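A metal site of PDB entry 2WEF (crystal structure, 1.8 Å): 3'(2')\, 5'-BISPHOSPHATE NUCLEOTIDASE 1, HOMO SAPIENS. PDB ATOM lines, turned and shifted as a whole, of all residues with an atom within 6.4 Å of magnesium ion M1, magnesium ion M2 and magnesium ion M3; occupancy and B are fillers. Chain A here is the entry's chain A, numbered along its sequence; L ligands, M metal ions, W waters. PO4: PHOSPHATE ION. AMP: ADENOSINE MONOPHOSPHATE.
The backbone NH of Gly 216 is in hydrogen-bond range of an oxygen (O3P) of AMP L2, at 2.8 Å.
N of Asp 116 is in hydrogen-bond range of O of Thr 130, 2.8 Å away. The backbone NH of Leu 132 sits at hydrogen-bond distance from the backbone carbonyl oxygen of Asp 113. The backbone carbonyl oxygen (O) of Leu 115 sits close to the side-chain hydroxyl (OG1) of Thr 118 (3.3 Å). The backbone NH (N) of Ala 217 sits at hydrogen-bond distance from the side-chain carboxylate (OD2) of Asp 116. The backbone carbonyl oxygen (O) of Asp 41 sits at hydrogen-bond distance from the backbone NH (N) of Lys 36 (2.7 Å).
Along chain A the residues within 4 Å of magnesium ion M1 span positions 70 to 116. The nearest printed residue that does not touch magnesium ion M1 is Asp 47 (4.01 Å).
Three residues have an atom within 4 Å of magnesium ion M2: Asp 113, Asp 116 and Asp 243. The nearest printed residue that does not touch magnesium ion M2 is Glu 70 (4.05 Å).
Asp 41 touches magnesium ion M3. The nearest printed residue that does not touch magnesium ion M3 is Lys 36 (4.1 Å).
Magnesium ion M1 is bound by the side-chain carboxylate of Glu 70 (2.1 Å), the side-chain carboxylate of Asp 113 (2.1 Å), the backbone carbonyl oxygen of Leu 115 (2.1 Å), water W4 (2.1 Å), an oxygen (O3) of PO4 L1 (2.1 Å) and an oxygen (O4) of PO4 L1 (2.2 Å). Magnesium ion M1 has six donor atoms within binding distance.
Magnesium ion M2 is bound by O3 of PO4 L1. Magnesium ion M2 is bound by OD1 of Asp 243 (2.0 Å). OD1 of Asp 116 is bound to magnesium ion M2 (2.1 Å). Magnesium ion M2 is bound by OD2 of Asp 113 (2.1 Å). Magnesium ion M2 is bound by water W3. O3' of AMP L2 binds magnesium ion M2, 2.3 Å away. Magnesium ion M2 has six donor atoms within binding distance.
Magnesium ion M3 is bound by O1 of PO4 L1 (2.0 Å). Magnesium ion M3 is bound by OE2 of Glu 70, 2.0 Å away. Water W2 binds magnesium ion M3, 2.1 Å away. Water W1 binds magnesium ion M3 (2.1 Å). Water W6 binds magnesium ion M3 (2.1 Å). Water W5 is bound to magnesium ion M3 (2.2 Å). Magnesium ion M3 has six donor atoms within binding distance.
Water W4 bridges the side-chain carboxylate (OD2) of Asp 47 (2.7 Å) and the side-chain carboxylate (OE2) of Glu 71 (2.7 Å). Water W3 bridges OD2 of Asp 243 (2.7 Å) and NE1 of Trp 242 (2.9 Å). Water W6 lies within hydrogen-bond range of the backbone carbonyl oxygen of Leu 42 (2.9 Å), the side-chain carboxylate of Glu 71 (3.0 Å) and the side-chain amino group of Lys 36 (3.2 Å). Water W1 bridges the side-chain carboxylate (OD1) of Asp 41 (2.7 Å) and the side-chain amino group (NZ) of Lys 36 (2.9 Å).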
ATOM      1  N   LYS A  36      25.066  -9.186 -23.412  1.00  0.00           N
ATOM      2  CA  LYS A  36      24.163  -8.904 -22.287  1.00  0.00           C
ATOM      3  C   LYS A  36      25.015  -9.044 -21.019  1.00  0.00           C
ATOM      4  O   LYS A  36      25.763  -8.114 -20.715  1.00  0.00           O
ATOM      5  CB  LYS A  36      22.926  -9.750 -22.323  1.00  0.00           C
ATOM      6  CG  LYS A  36      22.037  -9.261 -23.518  1.00  0.00           C
ATOM      7  CD  LYS A  36      20.626  -9.839 -23.593  1.00  0.00           C
ATOM      8  CE  LYS A  36      20.587 -11.330 -23.603  1.00  0.00           C
ATOM      9  NZ  LYS A  36      19.201 -11.774 -23.343  1.00  0.00           N
ATOM     10  N   ASP A  41      26.707 -14.516 -23.558  1.00  0.00           N
ATOM     11  CA  ASP A  41      25.270 -14.198 -23.315  1.00  0.00           C
ATOM     12  C   ASP A  41      24.942 -13.081 -24.317  1.00  0.00           C
ATOM     13  O   ASP A  41      25.034 -11.864 -23.986  1.00  0.00           O
ATOM     14  CB  ASP A  41      25.067 -13.774 -21.833  1.00  0.00           C
ATOM     15  CG  ASP A  41      23.621 -13.369 -21.459  1.00  0.00           C
ATOM     16  OD1 ASP A  41      22.660 -13.839 -22.135  1.00  0.00           O
ATOM     17  OD2 ASP A  41      23.442 -12.534 -20.499  1.00  0.00           O
ATOM     18  N   LEU A  42      24.532 -13.473 -25.543  1.00  0.00           N
ATOM     19  CA  LEU A  42      24.411 -12.521 -26.635  1.00  0.00           C
ATOM     20  C   LEU A  42      22.979 -12.297 -27.141  1.00  0.00           C
ATOM     21  O   LEU A  42      22.061 -13.154 -26.912  1.00  0.00           O
ATOM     22  CB  LEU A  42      25.274 -13.003 -27.823  1.00  0.00           C
ATOM     23  CG  LEU A  42      26.761 -13.191 -27.582  1.00  0.00           C
ATOM     24  CD1 LEU A  42      27.533 -13.587 -28.818  1.00  0.00           C
ATOM     25  CD2 LEU A  42      27.372 -11.907 -26.902  1.00  0.00           C
ATOM     26  N   ASP A  47      17.515 -12.100 -32.902  1.00  0.00           N
ATOM     27  CA  ASP A  47      16.791 -12.270 -31.637  1.00  0.00           C
ATOM     28  C   ASP A  47      15.746 -11.215 -31.492  1.00  0.00           C
ATOM     29  O   ASP A  47      14.593 -11.479 -31.167  1.00  0.00           O
ATOM     30  CB  ASP A  47      17.659 -12.279 -30.418  1.00  0.00           C
ATOM     31  CG  ASP A  47      18.785 -13.350 -30.460  1.00  0.00           C
ATOM     32  OD1 ASP A  47      19.797 -13.096 -31.139  1.00  0.00           O
ATOM     33  OD2 ASP A  47      18.684 -14.419 -29.824  1.00  0.00           O
ATOM     34  N   GLU A  70      12.080 -14.151 -24.078  1.00  0.00           N
ATOM     35  CA  GLU A  70      13.386 -14.023 -23.445  1.00  0.00           C
ATOM     36  C   GLU A  70      13.957 -12.606 -23.350  1.00  0.00           C
ATOM     37  O   GLU A  70      14.467 -12.176 -22.276  1.00  0.00           O
ATOM     38  CB  GLU A  70      14.394 -14.843 -24.215  1.00  0.00           C
ATOM     39  CG  GLU A  70      15.773 -14.788 -23.642  1.00  0.00           C
ATOM     40  CD  GLU A  70      16.813 -15.549 -24.384  1.00  0.00           C
ATOM     41  OE1 GLU A  70      16.517 -16.154 -25.412  1.00  0.00           O
ATOM     42  OE2 GLU A  70      17.933 -15.610 -23.859  1.00  0.00           O
ATOM     43  N   GLU A  71      13.885 -11.885 -24.459  1.00  0.00           N
ATOM     44  CA  GLU A  71      14.580 -10.625 -24.613  1.00  0.00           C
ATOM     45  C   GLU A  71      13.773  -9.498 -23.948  1.00  0.00           C
ATOM     46  O   GLU A  71      12.547  -9.453 -24.012  1.00  0.00           O
ATOM     47  CB  GLU A  71      14.860 -10.330 -26.068  1.00  0.00           C
ATOM     48  CG  GLU A  71      15.647 -11.460 -26.782  1.00  0.00           C
ATOM     49  CD  GLU A  71      16.986 -11.887 -26.166  1.00  0.00           C
ATOM     50  OE1 GLU A  71      17.736 -11.042 -25.540  1.00  0.00           O
ATOM     51  OE2 GLU A  71      17.339 -13.080 -26.346  1.00  0.00           O
ATOM     52  N   ASP A 113      11.219 -18.301 -26.914  1.00  0.00           N
ATOM     53  CA  ASP A 113      12.599 -18.105 -27.156  1.00  0.00           C
ATOM     54  C   ASP A 113      12.732 -17.844 -28.608  1.00  0.00           C
ATOM     55  O   ASP A 113      12.602 -18.747 -29.408  1.00  0.00           O
ATOM     56  CB  ASP A 113      13.439 -19.311 -26.723  1.00  0.00           C
ATOM     57  CG  ASP A 113      14.926 -18.969 -26.676  1.00  0.00           C
ATOM     58  OD1 ASP A 113      15.359 -18.016 -27.329  1.00  0.00           O
ATOM     59  OD2 ASP A 113      15.614 -19.713 -25.987  1.00  0.00           O
ATOM     60  N   PRO A 114      12.952 -16.572 -28.953  1.00  0.00           N
ATOM     61  CA  PRO A 114      12.846 -16.178 -30.357  1.00  0.00           C
ATOM     62  C   PRO A 114      13.979 -16.694 -31.170  1.00  0.00           C
ATOM     63  O   PRO A 114      13.882 -16.795 -32.402  1.00  0.00           O
ATOM     64  CB  PRO A 114      12.848 -14.637 -30.268  1.00  0.00           C
ATOM     65  CG  PRO A 114      13.673 -14.306 -29.041  1.00  0.00           C
ATOM     66  CD  PRO A 114      13.236 -15.434 -28.066  1.00  0.00           C
ATOM     67  N   LEU A 115      15.088 -17.007 -30.500  1.00  0.00           N
ATOM     68  CA  LEU A 115      16.271 -17.608 -31.148  1.00  0.00           C
ATOM     69  C   LEU A 115      17.021 -18.262 -30.010  1.00  0.00           C
ATOM     70  O   LEU A 115      17.535 -17.572 -29.131  1.00  0.00           O
ATOM     71  CB  LEU A 115      17.133 -16.540 -31.871  1.00  0.00           C
ATOM     72  CG  LEU A 115      18.105 -17.044 -32.881  1.00  0.00           C
ATOM     73  CD1 LEU A 115      18.771 -15.840 -33.639  1.00  0.00           C
ATOM     74  CD2 LEU A 115      19.180 -17.951 -32.212  1.00  0.00           C
ATOM     75  N   ASP A 116      17.075 -19.580 -30.031  1.00  0.00           N
ATOM     76  CA  ASP A 116      17.784 -20.395 -29.061  1.00  0.00           C
ATOM     77  C   ASP A 116      19.008 -20.930 -29.689  1.00  0.00           C
ATOM     78  O   ASP A 116      18.952 -21.546 -30.767  1.00  0.00           O
ATOM     79  CB  ASP A 116      16.908 -21.543 -28.474  1.00  0.00           C
ATOM     80  CG  ASP A 116      17.633 -22.317 -27.398  1.00  0.00           C
ATOM     81  OD1 ASP A 116      17.968 -21.660 -26.378  1.00  0.00           O
ATOM     82  OD2 ASP A 116      17.809 -23.570 -27.584  1.00  0.00           O
ATOM     83  N   GLY A 117      20.152 -20.695 -29.019  1.00  0.00           N
ATOM     84  CA  GLY A 117      21.458 -20.991 -29.551  1.00  0.00           C
ATOM     85  C   GLY A 117      22.125 -19.806 -30.215  1.00  0.00           C
ATOM     86  O   GLY A 117      22.930 -19.944 -31.157  1.00  0.00           O
ATOM     87  N   THR A 118      21.869 -18.623 -29.674  1.00  0.00           N
ATOM     88  CA  THR A 118      22.412 -17.387 -30.231  1.00  0.00           C
ATOM     89  C   THR A 118      23.978 -17.344 -30.315  1.00  0.00           C
ATOM     90  O   THR A 118      24.577 -16.867 -31.321  1.00  0.00           O
ATOM     91  CB  THR A 118      21.888 -16.199 -29.429  1.00  0.00           C
ATOM     92  OG1 THR A 118      20.478 -16.173 -29.369  1.00  0.00           O
ATOM     93  CG2 THR A 118      22.447 -14.874 -29.989  1.00  0.00           C
ATOM     94  N   THR A 130      17.268 -22.945 -32.797  1.00  0.00           N
ATOM     95  CA  THR A 130      15.821 -23.173 -32.908  1.00  0.00           C
ATOM     96  C   THR A 130      15.058 -21.882 -32.543  1.00  0.00           C
ATOM     97  O   THR A 130      15.584 -21.001 -31.863  1.00  0.00           O
ATOM     98  CB  THR A 130      15.351 -24.358 -32.047  1.00  0.00           C
ATOM     99  OG1 THR A 130      15.757 -24.138 -30.696  1.00  0.00           O
ATOM    100  CG2 THR A 130      15.928 -25.733 -32.598  1.00  0.00           C
ATOM    101  N   LEU A 132      11.581 -21.297 -30.398  1.00  0.00           N
ATOM    102  CA  LEU A 132      10.753 -22.037 -29.466  1.00  0.00           C
ATOM    103  C   LEU A 132       9.499 -21.264 -29.053  1.00  0.00           C
ATOM    104  O   LEU A 132       9.562 -20.175 -28.485  1.00  0.00           O
ATOM    105  CB  LEU A 132      11.561 -22.452 -28.208  1.00  0.00           C
ATOM    106  CG  LEU A 132      12.924 -23.124 -28.444  1.00  0.00           C
ATOM    107  CD1 LEU A 132      13.799 -23.327 -27.143  1.00  0.00           C
ATOM    108  CD2 LEU A 132      12.768 -24.445 -29.252  1.00  0.00           C
ATOM    109  N   GLY A 216      22.201 -24.904 -27.732  1.00  0.00           N
ATOM    110  CA  GLY A 216      20.751 -24.857 -27.786  1.00  0.00           C
ATOM    111  C   GLY A 216      20.039 -25.939 -27.006  1.00  0.00           C
ATOM    112  O   GLY A 216      20.378 -27.144 -27.075  1.00  0.00           O
ATOM    113  N   ALA A 217      19.074 -25.511 -26.193  1.00  0.00           N
ATOM    114  CA  ALA A 217      18.138 -26.422 -25.512  1.00  0.00           C
ATOM    115  C   ALA A 217      17.195 -27.130 -26.530  1.00  0.00           C
ATOM    116  O   ALA A 217      16.953 -28.337 -26.414  1.00  0.00           O
ATOM    117  CB  ALA A 217      17.324 -25.653 -24.445  1.00  0.00           C
ATOM    118  N   TRP A 242      11.486 -20.515 -21.096  1.00  0.00           N
ATOM    119  CA  TRP A 242      11.337 -20.502 -22.568  1.00  0.00           C
ATOM    120  C   TRP A 242      12.265 -21.485 -23.327  1.00  0.00           C
ATOM    121  O   TRP A 242      11.981 -21.856 -24.491  1.00  0.00           O
ATOM    122  CB  TRP A 242      11.471 -19.059 -23.128  1.00  0.00           C
ATOM    123  CG  TRP A 242      12.669 -18.330 -22.611  1.00  0.00           C
ATOM    124  CD1 TRP A 242      13.999 -18.524 -22.962  1.00  0.00           C
ATOM    125  CD2 TRP A 242      12.661 -17.324 -21.602  1.00  0.00           C
ATOM    126  NE1 TRP A 242      14.815 -17.695 -22.214  1.00  0.00           N
ATOM    127  CE2 TRP A 242      14.021 -16.937 -21.370  1.00  0.00           C
ATOM    128  CE3 TRP A 242      11.652 -16.652 -20.903  1.00  0.00           C
ATOM    129  CZ2 TRP A 242      14.373 -15.964 -20.456  1.00  0.00           C
ATOM    130  CZ3 TRP A 242      12.004 -15.669 -19.995  1.00  0.00           C
ATOM    131  CH2 TRP A 242      13.379 -15.352 -19.747  1.00  0.00           C
ATOM    132  N   ASP A 243      13.370 -21.917 -22.693  1.00  0.00           N
ATOM    133  CA  ASP A 243      14.294 -22.907 -23.264  1.00  0.00           C
ATOM    134  C   ASP A 243      13.705 -24.296 -23.169  1.00  0.00           C
ATOM    135  O   ASP A 243      13.987 -25.180 -24.007  1.00  0.00           O
ATOM    136  CB  ASP A 243      15.640 -22.879 -22.453  1.00  0.00           C
ATOM    137  CG  ASP A 243      16.425 -21.633 -22.705  1.00  0.00           C
ATOM    138  OD1 ASP A 243      16.767 -21.457 -23.862  1.00  0.00           O
ATOM    139  OD2 ASP A 243      16.669 -20.835 -21.761  1.00  0.00           O
HETATM  140  P   PO4 L   1      19.595 -17.887 -26.309  1.00  0.00           P
HETATM  141  O1  PO4 L   1      20.095 -17.486 -24.912  1.00  0.00           O
HETATM  142  O2  PO4 L   1      20.659 -18.720 -27.039  1.00  0.00           O
HETATM  143  O3  PO4 L   1      18.199 -18.580 -26.236  1.00  0.00           O
HETATM  144  O4  PO4 L   1      19.310 -16.515 -27.070  1.00  0.00           O
HETATM  145  P   AMP L   2      23.385 -24.156 -24.083  1.00  0.00           P
HETATM  146  O1P AMP L   2      23.307 -25.657 -23.911  1.00  0.00           O
HETATM  147  O2P AMP L   2      24.606 -23.622 -23.443  1.00  0.00           O
HETATM  148  O3P AMP L   2      23.119 -23.605 -25.440  1.00  0.00           O
HETATM  149  O5' AMP L   2      22.256 -23.576 -23.121  1.00  0.00           O
HETATM  150  C5' AMP L   2      20.855 -23.776 -23.379  1.00  0.00           C
HETATM  151  C4' AMP L   2      20.090 -22.462 -23.305  1.00  0.00           C
HETATM  152  O4' AMP L   2      20.219 -21.870 -22.031  1.00  0.00           O
HETATM  153  C3' AMP L   2      20.614 -21.320 -24.231  1.00  0.00           C
HETATM  154  O3' AMP L   2      19.632 -20.229 -24.330  1.00  0.00           O
HETATM  155  C2' AMP L   2      21.653 -20.633 -23.458  1.00  0.00           C
HETATM  156  O2' AMP L   2      21.924 -19.330 -23.965  1.00  0.00           O
HETATM  157  C1' AMP L   2      20.947 -20.649 -22.108  1.00  0.00           C
HETATM  158  N9  AMP L   2      22.014 -20.655 -21.133  1.00  0.00           N
HETATM  159  C8  AMP L   2      22.561 -21.727 -20.540  1.00  0.00           C
HETATM  160  N7  AMP L   2      23.494 -21.359 -19.665  1.00  0.00           N
HETATM  161  C5  AMP L   2      23.587 -20.007 -19.757  1.00  0.00           C
HETATM  162  C6  AMP L   2      24.397 -18.958 -19.128  1.00  0.00           C
HETATM  163  N6  AMP L   2      25.343 -19.264 -18.237  1.00  0.00           N
HETATM  164  N1  AMP L   2      24.151 -17.671 -19.499  1.00  0.00           N
HETATM  165  C2  AMP L   2      23.209 -17.344 -20.391  1.00  0.00           C
HETATM  166  N3  AMP L   2      22.424 -18.246 -20.996  1.00  0.00           N
HETATM  167  C4  AMP L   2      22.584 -19.558 -20.693  1.00  0.00           C
HETATM  168 MG    MG M   1      17.154 -17.011 -27.167  1.00  0.00          MG
HETATM  169 MG    MG M   2      17.493 -20.076 -25.165  1.00  0.00          MG
HETATM  170 MG    MG M   3      19.942 -15.778 -23.880  1.00  0.00          MG
HETATM  171  O   HOH W   1      20.055 -14.346 -22.400  1.00  0.00           O
HETATM  172  O   HOH W   2      21.987 -15.744 -23.655  1.00  0.00           O
HETATM  173  O   HOH W   3      17.329 -18.718 -23.355  1.00  0.00           O
HETATM  174  O   HOH W   4      16.792 -15.153 -28.050  1.00  0.00           O
HETATM  175  O   HOH W   5      19.823 -17.190 -22.184  1.00  0.00           O
HETATM  176  O   HOH W   6      19.898 -14.216 -25.341  1.00  0.00           O
